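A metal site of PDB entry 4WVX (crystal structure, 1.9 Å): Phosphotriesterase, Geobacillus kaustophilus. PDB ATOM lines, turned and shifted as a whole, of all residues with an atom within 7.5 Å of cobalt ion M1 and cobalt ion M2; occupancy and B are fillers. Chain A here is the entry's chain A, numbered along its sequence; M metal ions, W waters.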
ATOM      1  N   HIS A  23      30.157  19.637 -14.765  1.00  0.00           N
ATOM      2  CA  HIS A  23      28.886  19.187 -15.367  1.00  0.00           C
ATOM      3  C   HIS A  23      27.699  19.950 -14.826  1.00  0.00           C
ATOM      4  O   HIS A  23      27.128  19.564 -13.802  1.00  0.00           O
ATOM      5  CB  HIS A  23      28.701  17.702 -15.097  1.00  0.00           C
ATOM      6  CG  HIS A  23      27.650  17.044 -15.943  1.00  0.00           C
ATOM      7  ND1 HIS A  23      27.909  15.886 -16.638  1.00  0.00           N
ATOM      8  CD2 HIS A  23      26.360  17.345 -16.187  1.00  0.00           C
ATOM      9  CE1 HIS A  23      26.832  15.500 -17.275  1.00  0.00           C
ATOM     10  NE2 HIS A  23      25.863  16.367 -17.018  1.00  0.00           N
ATOM     11  N   GLU A  24      27.317  21.018 -15.527  1.00  0.00           N
ATOM     12  CA  GLU A  24      26.102  21.764 -15.184  1.00  0.00           C
ATOM     13  C   GLU A  24      25.409  22.214 -16.449  1.00  0.00           C
ATOM     14  O   GLU A  24      26.057  22.444 -17.461  1.00  0.00           O
ATOM     15  CB  GLU A  24      26.423  23.009 -14.361  1.00  0.00           C
ATOM     16  CG  GLU A  24      27.353  22.811 -13.164  1.00  0.00           C
ATOM     17  CD  GLU A  24      26.688  22.135 -11.979  1.00  0.00           C
ATOM     18  OE1 GLU A  24      25.441  22.116 -11.882  1.00  0.00           O
ATOM     19  OE2 GLU A  24      27.447  21.603 -11.143  1.00  0.00           O
ATOM     20  N   HIS A  25      24.088  22.360 -16.393  1.00  0.00           N
ATOM     21  CA  HIS A  25      23.317  22.901 -17.523  1.00  0.00           C
ATOM     22  C   HIS A  25      22.715  24.261 -17.267  1.00  0.00           C
ATOM     23  O   HIS A  25      21.950  24.449 -16.316  1.00  0.00           O
ATOM     24  CB  HIS A  25      22.174  21.984 -17.931  1.00  0.00           C
ATOM     25  CG  HIS A  25      22.626  20.596 -18.180  1.00  0.00           C
ATOM     26  ND1 HIS A  25      23.125  20.180 -19.394  1.00  0.00           N
ATOM     27  CD2 HIS A  25      22.710  19.533 -17.355  1.00  0.00           C
ATOM     28  CE1 HIS A  25      23.476  18.912 -19.313  1.00  0.00           C
ATOM     29  NE2 HIS A  25      23.246  18.499 -18.077  1.00  0.00           N
ATOM     30  N   PHE A  28      18.207  23.166 -20.443  1.00  0.00           N
ATOM     31  CA  PHE A  28      18.017  21.776 -20.810  1.00  0.00           C
ATOM     32  C   PHE A  28      16.558  21.522 -21.110  1.00  0.00           C
ATOM     33  O   PHE A  28      15.691  22.037 -20.394  1.00  0.00           O
ATOM     34  CB  PHE A  28      18.491  20.859 -19.671  1.00  0.00           C
ATOM     35  CG  PHE A  28      18.462  19.398 -20.030  1.00  0.00           C
ATOM     36  CD1 PHE A  28      17.310  18.661 -19.849  1.00  0.00           C
ATOM     37  CD2 PHE A  28      19.580  18.773 -20.557  1.00  0.00           C
ATOM     38  CE1 PHE A  28      17.259  17.332 -20.196  1.00  0.00           C
ATOM     39  CE2 PHE A  28      19.538  17.433 -20.906  1.00  0.00           C
ATOM     40  CZ  PHE A  28      18.367  16.717 -20.720  1.00  0.00           C
ATOM     41  N   ASP A  68      29.344  22.698 -19.708  1.00  0.00           N
ATOM     42  CA  ASP A  68      27.924  22.534 -19.924  1.00  0.00           C
ATOM     43  C   ASP A  68      27.789  21.535 -21.103  1.00  0.00           C
ATOM     44  O   ASP A  68      27.927  21.829 -22.218  1.00  0.00           O
ATOM     45  CB  ASP A  68      27.223  23.863 -20.156  1.00  0.00           C
ATOM     46  CG  ASP A  68      25.728  23.714 -20.508  1.00  0.00           C
ATOM     47  OD1 ASP A  68      25.341  22.686 -21.082  1.00  0.00           O
ATOM     48  OD2 ASP A  68      24.989  24.619 -20.208  1.00  0.00           O
ATOM     49  N   PRO A  69      27.487  20.314 -20.729  1.00  0.00           N
ATOM     50  CA  PRO A  69      27.489  19.218 -21.673  1.00  0.00           C
ATOM     51  C   PRO A  69      26.052  18.935 -22.181  1.00  0.00           C
ATOM     52  O   PRO A  69      25.722  17.818 -22.360  1.00  0.00           O
ATOM     53  CB  PRO A  69      28.055  18.072 -20.854  1.00  0.00           C
ATOM     54  CG  PRO A  69      27.533  18.296 -19.510  1.00  0.00           C
ATOM     55  CD  PRO A  69      27.384  19.812 -19.365  1.00  0.00           C
ATOM     56  N   THR A  70      25.225  19.953 -22.326  1.00  0.00           N
ATOM     57  CA  THR A  70      23.871  19.772 -22.839  1.00  0.00           C
ATOM     58  C   THR A  70      23.939  19.113 -24.226  1.00  0.00           C
ATOM     59  O   THR A  70      24.583  19.649 -25.126  1.00  0.00           O
ATOM     60  CB  THR A  70      23.126  21.110 -22.946  1.00  0.00           C
ATOM     61  OG1 THR A  70      23.063  21.718 -21.649  1.00  0.00           O
ATOM     62  CG2 THR A  70      21.723  20.886 -23.414  1.00  0.00           C
ATOM     63  N   PRO A  71      23.293  17.945 -24.387  1.00  0.00           N
ATOM     64  CA  PRO A  71      23.307  17.281 -25.706  1.00  0.00           C
ATOM     65  C   PRO A  71      22.632  18.064 -26.819  1.00  0.00           C
ATOM     66  O   PRO A  71      21.717  18.855 -26.570  1.00  0.00           O
ATOM     67  CB  PRO A  71      22.522  16.001 -25.463  1.00  0.00           C
ATOM     68  CG  PRO A  71      22.692  15.724 -24.003  1.00  0.00           C
ATOM     69  CD  PRO A  71      22.655  17.092 -23.369  1.00  0.00           C
ATOM     70  N   TYR A  99      22.091  12.549 -26.736  1.00  0.00           N
ATOM     71  CA  TYR A  99      21.795  11.900 -25.472  1.00  0.00           C
ATOM     72  C   TYR A  99      21.564  10.392 -25.648  1.00  0.00           C
ATOM     73  O   TYR A  99      21.625   9.874 -26.766  1.00  0.00           O
ATOM     74  CB  TYR A  99      20.559  12.543 -24.892  1.00  0.00           C
ATOM     75  CG  TYR A  99      20.427  12.541 -23.407  1.00  0.00           C
ATOM     76  CD1 TYR A  99      21.518  12.623 -22.522  1.00  0.00           C
ATOM     77  CD2 TYR A  99      19.161  12.492 -22.882  1.00  0.00           C
ATOM     78  CE1 TYR A  99      21.292  12.648 -21.139  1.00  0.00           C
ATOM     79  CE2 TYR A  99      18.927  12.519 -21.540  1.00  0.00           C
ATOM     80  CZ  TYR A  99      19.970  12.592 -20.669  1.00  0.00           C
ATOM     81  OH  TYR A  99      19.605  12.582 -19.332  1.00  0.00           O
ATOM     82  N   TYR A 100      21.337   9.670 -24.546  1.00  0.00           N
ATOM     83  CA  TYR A 100      21.115   8.226 -24.635  1.00  0.00           C
ATOM     84  C   TYR A 100      19.745   7.941 -25.251  1.00  0.00           C
ATOM     85  O   TYR A 100      18.853   8.793 -25.298  1.00  0.00           O
ATOM     86  CB  TYR A 100      21.325   7.513 -23.280  1.00  0.00           C
ATOM     87  CG  TYR A 100      20.228   7.672 -22.272  1.00  0.00           C
ATOM     88  CD1 TYR A 100      20.067   8.846 -21.559  1.00  0.00           C
ATOM     89  CD2 TYR A 100      19.366   6.603 -21.987  1.00  0.00           C
ATOM     90  CE1 TYR A 100      19.052   8.961 -20.627  1.00  0.00           C
ATOM     91  CE2 TYR A 100      18.355   6.713 -21.063  1.00  0.00           C
ATOM     92  CZ  TYR A 100      18.209   7.896 -20.374  1.00  0.00           C
ATOM     93  OH  TYR A 100      17.211   8.007 -19.446  1.00  0.00           O
ATOM     94  N   KCX A 145      30.128  14.857 -25.815  1.00  0.00           N
ATOM     95  CA  KCX A 145      29.237  14.218 -24.828  1.00  0.00           C
ATOM     96  CB  KCX A 145      28.070  15.167 -24.562  1.00  0.00           C
ATOM     97  CG  KCX A 145      26.958  14.535 -23.740  1.00  0.00           C
ATOM     98  CD  KCX A 145      27.418  14.276 -22.323  1.00  0.00           C
ATOM     99  CE  KCX A 145      26.296  13.783 -21.440  1.00  0.00           C
ATOM    100  NZ  KCX A 145      25.481  14.897 -21.011  1.00  0.00           N
ATOM    101  C   KCX A 145      28.718  12.910 -25.347  1.00  0.00           C
ATOM    102  O   KCX A 145      28.193  12.842 -26.460  1.00  0.00           O
ATOM    103  CX  KCX A 145      24.699  14.794 -19.944  1.00  0.00           C
ATOM    104  OQ1 KCX A 145      24.598  13.771 -19.289  1.00  0.00           O
ATOM    105  OQ2 KCX A 145      23.987  15.843 -19.583  1.00  0.00           O
ATOM    106  N   LEU A 146      28.845  11.871 -24.544  1.00  0.00           N
ATOM    107  CA  LEU A 146      28.353  10.538 -24.853  1.00  0.00           C
ATOM    108  C   LEU A 146      27.410  10.107 -23.765  1.00  0.00           C
ATOM    109  O   LEU A 146      27.532  10.548 -22.616  1.00  0.00           O
ATOM    110  CB  LEU A 146      29.525   9.539 -24.928  1.00  0.00           C
ATOM    111  CG  LEU A 146      30.494   9.676 -26.089  1.00  0.00           C
ATOM    112  CD1 LEU A 146      31.588   8.596 -25.986  1.00  0.00           C
ATOM    113  CD2 LEU A 146      29.751   9.618 -27.417  1.00  0.00           C
ATOM    114  N   ALA A 147      26.498   9.215 -24.110  1.00  0.00           N
ATOM    115  CA  ALA A 147      25.548   8.745 -23.123  1.00  0.00           C
ATOM    116  C   ALA A 147      25.098   7.327 -23.403  1.00  0.00           C
ATOM    117  O   ALA A 147      24.879   6.962 -24.550  1.00  0.00           O
ATOM    118  CB  ALA A 147      24.373   9.678 -23.109  1.00  0.00           C
ATOM    119  N   THR A 177      30.893  11.662 -20.271  1.00  0.00           N
ATOM    120  CA  THR A 177      29.776  10.723 -20.447  1.00  0.00           C
ATOM    121  C   THR A 177      28.679  10.873 -19.396  1.00  0.00           C
ATOM    122  O   THR A 177      28.873  11.449 -18.311  1.00  0.00           O
ATOM    123  CB  THR A 177      30.191   9.237 -20.456  1.00  0.00           C
ATOM    124  OG1 THR A 177      30.362   8.759 -19.109  1.00  0.00           O
ATOM    125  CG2 THR A 177      31.451   8.988 -21.286  1.00  0.00           C
ATOM    126  N   HIS A 178      27.524  10.318 -19.767  1.00  0.00           N
ATOM    127  CA  HIS A 178      26.376  10.072 -18.930  1.00  0.00           C
ATOM    128  C   HIS A 178      26.293   8.560 -18.776  1.00  0.00           C
ATOM    129  O   HIS A 178      26.327   7.838 -19.770  1.00  0.00           O
ATOM    130  CB  HIS A 178      25.143  10.620 -19.656  1.00  0.00           C
ATOM    131  CG  HIS A 178      23.829  10.109 -19.170  1.00  0.00           C
ATOM    132  ND1 HIS A 178      22.916  10.929 -18.543  1.00  0.00           N
ATOM    133  CD2 HIS A 178      23.224   8.901 -19.291  1.00  0.00           C
ATOM    134  CE1 HIS A 178      21.828  10.243 -18.256  1.00  0.00           C
ATOM    135  NE2 HIS A 178      21.990   9.008 -18.699  1.00  0.00           N
ATOM    136  N   THR A 179      26.281   8.088 -17.529  1.00  0.00           N
ATOM    137  CA  THR A 179      25.819   6.734 -17.225  1.00  0.00           C
ATOM    138  C   THR A 179      24.422   6.794 -16.632  1.00  0.00           C
ATOM    139  O   THR A 179      24.084   7.723 -15.868  1.00  0.00           O
ATOM    140  CB  THR A 179      26.745   6.010 -16.245  1.00  0.00           C
ATOM    141  OG1 THR A 179      26.832   6.727 -15.016  1.00  0.00           O
ATOM    142  CG2 THR A 179      28.114   5.856 -16.867  1.00  0.00           C
ATOM    143  N   GLN A 180      23.598   5.806 -16.971  1.00  0.00           N
ATOM    144  CA  GLN A 180      22.210   5.787 -16.535  1.00  0.00           C
ATOM    145  C   GLN A 180      22.048   4.864 -15.313  1.00  0.00           C
ATOM    146  O   GLN A 180      22.390   3.675 -15.356  1.00  0.00           O
ATOM    147  CB  GLN A 180      21.300   5.331 -17.679  1.00  0.00           C
ATOM    148  CG  GLN A 180      19.803   5.401 -17.426  1.00  0.00           C
ATOM    149  CD  GLN A 180      19.232   6.775 -17.154  1.00  0.00           C
ATOM    150  OE1 GLN A 180      19.811   7.818 -17.485  1.00  0.00           O
ATOM    151  NE2 GLN A 180      18.038   6.776 -16.569  1.00  0.00           N
ATOM    152  N   GLY A 205      30.744   9.857 -16.393  1.00  0.00           N
ATOM    153  CA  GLY A 205      29.841  10.665 -15.596  1.00  0.00           C
ATOM    154  C   GLY A 205      28.800   9.887 -14.818  1.00  0.00           C
ATOM    155  O   GLY A 205      28.542   8.709 -15.079  1.00  0.00           O
ATOM    156  N   HIS A 206      28.169  10.609 -13.899  1.00  0.00           N
ATOM    157  CA  HIS A 206      27.114  10.118 -13.016  1.00  0.00           C
ATOM    158  C   HIS A 206      27.504   8.889 -12.254  1.00  0.00           C
ATOM    159  O   HIS A 206      26.662   8.037 -11.968  1.00  0.00           O
ATOM    160  CB  HIS A 206      25.787   9.884 -13.768  1.00  0.00           C
ATOM    161  CG  HIS A 206      25.367  11.029 -14.615  1.00  0.00           C
ATOM    162  ND1 HIS A 206      25.699  12.340 -14.318  1.00  0.00           N
ATOM    163  CD2 HIS A 206      24.647  11.078 -15.775  1.00  0.00           C
ATOM    164  CE1 HIS A 206      25.197  13.145 -15.240  1.00  0.00           C
ATOM    165  NE2 HIS A 206      24.532  12.403 -16.117  1.00  0.00           N
ATOM    166  N   ASP A 229      28.715  13.819 -10.041  1.00  0.00           N
ATOM    167  CA  ASP A 229      28.301  15.049 -10.690  1.00  0.00           C
ATOM    168  C   ASP A 229      26.811  15.332 -10.549  1.00  0.00           C
ATOM    169  O   ASP A 229      26.306  16.210 -11.222  1.00  0.00           O
ATOM    170  CB  ASP A 229      28.736  15.035 -12.157  1.00  0.00           C
ATOM    171  CG  ASP A 229      28.238  13.830 -12.914  1.00  0.00           C
ATOM    172  OD1 ASP A 229      27.261  13.217 -12.443  1.00  0.00           O
ATOM    173  OD2 ASP A 229      28.803  13.501 -13.970  1.00  0.00           O
ATOM    174  N   ARG A 230      26.130  14.613  -9.652  1.00  0.00           N
ATOM    175  CA  ARG A 230      24.713  14.866  -9.391  1.00  0.00           C
ATOM    176  C   ARG A 230      24.369  15.168  -7.925  1.00  0.00           C
ATOM    177  O   ARG A 230      23.271  14.851  -7.456  1.00  0.00           O
ATOM    178  CB  ARG A 230      23.888  13.691  -9.877  1.00  0.00           C
ATOM    179  CG  ARG A 230      23.836  13.623 -11.380  1.00  0.00           C
ATOM    180  CD  ARG A 230      23.029  12.428 -11.872  1.00  0.00           C
ATOM    181  NE  ARG A 230      22.445  12.736 -13.182  1.00  0.00           N
ATOM    182  CZ  ARG A 230      21.709  11.900 -13.920  1.00  0.00           C
ATOM    183  NH1 ARG A 230      21.454  10.664 -13.506  1.00  0.00           N
ATOM    184  NH2 ARG A 230      21.241  12.310 -15.111  1.00  0.00           N
ATOM    185  N   HIS A 265      26.964  19.132  -9.851  1.00  0.00           N
ATOM    186  CA  HIS A 265      25.566  18.931  -9.496  1.00  0.00           C
ATOM    187  C   HIS A 265      24.638  18.508 -10.642  1.00  0.00           C
ATOM    188  O   HIS A 265      23.527  18.041 -10.359  1.00  0.00           O
ATOM    189  CB  HIS A 265      24.917  20.224  -8.960  1.00  0.00           C
ATOM    190  CG  HIS A 265      25.757  21.038  -8.020  1.00  0.00           C
ATOM    191  ND1 HIS A 265      26.653  21.984  -8.463  1.00  0.00           N
ATOM    192  CD2 HIS A 265      25.749  21.130  -6.677  1.00  0.00           C
ATOM    193  CE1 HIS A 265      27.206  22.591  -7.427  1.00  0.00           C
ATOM    194  NE2 HIS A 265      26.662  22.097  -6.328  1.00  0.00           N
ATOM    195  N   ASP A 266      25.008  18.751 -11.893  1.00  0.00           N
ATOM    196  CA  ASP A 266      24.130  18.438 -13.036  1.00  0.00           C
ATOM    197  C   ASP A 266      22.834  19.277 -12.952  1.00  0.00           C
ATOM    198  O   ASP A 266      21.752  18.809 -13.297  1.00  0.00           O
ATOM    199  CB  ASP A 266      23.846  16.920 -13.080  1.00  0.00           C
ATOM    200  CG  ASP A 266      23.288  16.418 -14.427  1.00  0.00           C
ATOM    201  OD1 ASP A 266      23.405  17.127 -15.428  1.00  0.00           O
ATOM    202  OD2 ASP A 266      22.752  15.298 -14.463  1.00  0.00           O
ATOM    203  N   THR A 267      22.961  20.525 -12.502  1.00  0.00           N
ATOM    204  CA  THR A 267      21.812  21.409 -12.424  1.00  0.00           C
ATOM    205  C   THR A 267      21.204  21.644 -13.799  1.00  0.00           C
ATOM    206  O   THR A 267      21.883  21.582 -14.834  1.00  0.00           O
ATOM    207  CB  THR A 267      22.103  22.789 -11.805  1.00  0.00           C
ATOM    208  OG1 THR A 267      23.180  23.453 -12.488  1.00  0.00           O
ATOM    209  CG2 THR A 267      22.379  22.642 -10.294  1.00  0.00           C
ATOM    210  N   VAL A 268      19.905  21.881 -13.764  1.00  0.00           N
ATOM    211  CA  VAL A 268      19.230  22.484 -14.880  1.00  0.00           C
ATOM    212  C   VAL A 268      18.707  23.832 -14.439  1.00  0.00           C
ATOM    213  O   VAL A 268      17.688  23.913 -13.746  1.00  0.00           O
ATOM    214  CB  VAL A 268      18.094  21.604 -15.382  1.00  0.00           C
ATOM    215  CG1 VAL A 268      17.320  22.302 -16.495  1.00  0.00           C
ATOM    216  CG2 VAL A 268      18.666  20.296 -15.889  1.00  0.00           C
HETATM  217 CO    CO M   1      23.330  12.989 -17.873  1.00  0.00          CO
HETATM  218 CO    CO M   2      23.701  16.477 -17.518  1.00  0.00          CO
HETATM  219  O   HOH W   1      22.822  14.747 -17.007  1.00  0.00           O
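The side-chain hydroxyl (OG1) of Thr 70 is in hydrogen-bond range of a ring nitrogen (ND1) of His 25, 2.7 Å away. A ring nitrogen (NE2) of His 178 sits at hydrogen-bond distance from the side-chain amide oxygen (OE1) of Gln 180 (2.8 Å). O of Leu 146 lies within hydrogen-bond range of N of His 178, 2.9 Å away. The side-chain hydroxyl of Thr 179 sits at hydrogen-bond distance from the backbone carbonyl oxygen of His 206, 3.3 Å away. ND1 of His 206 is in hydrogen-bond range of OD1 of Asp 229, at 2.6 Å. The side-chain carboxylate (OD2) of Asp 266 is in salt-bridge range of the guanidinium group (NE) of Arg 230 (2.9 Å). The backbone NH (N) of Asp 266 lies within hydrogen-bond range of the side-chain carboxylate (OE1) of Glu 24 (3.4 Å). The backbone carbonyl oxygen (O) of Asp 229 sits at hydrogen-bond distance from the backbone NH (N) of Asp 266 (2.9 Å).
CE1 of Tyr 99 touches cobalt ion M1 (3.9 Å). Arg 230 touches cobalt ion M1. Five residues have an atom within 4 Å of cobalt ion M1: Tyr 99, KCX 145, His 178, His 206 and Arg 230.
Within 4 Å of cobalt ion M2: His 23, His 25, KCX 145 and Asp 266. Along chain A the residues within 4 Å of cobalt ion M2 span positions 23 to 266. The nearest printed residue that does not touch cobalt ion M2 is His 206 (4.3 Å).
Cobalt ion M1 is bound by water W1 (2.0 Å), OQ1 of KCX 145 (2.1 Å), a ring nitrogen (ND1) of His 178 (2.2 Å) and a ring nitrogen (NE2) of His 206 (2.2 Å). Cobalt ion M1 has four donor atoms within binding distance.
Cobalt ion M2 is bound by water W1 (2.0 Å), a ring nitrogen (NE2) of His 25 (2.1 Å), OQ2 of KCX 145 (2.2 Å), the side-chain carboxylate of Asp 266 (2.2 Å) and a ring nitrogen (NE2) of His 23 (2.2 Å). Cobalt ion M2 has five donor atoms within binding distance.
Water W1 bridges OD2 of Asp 266 and NH2 of Arg 230.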
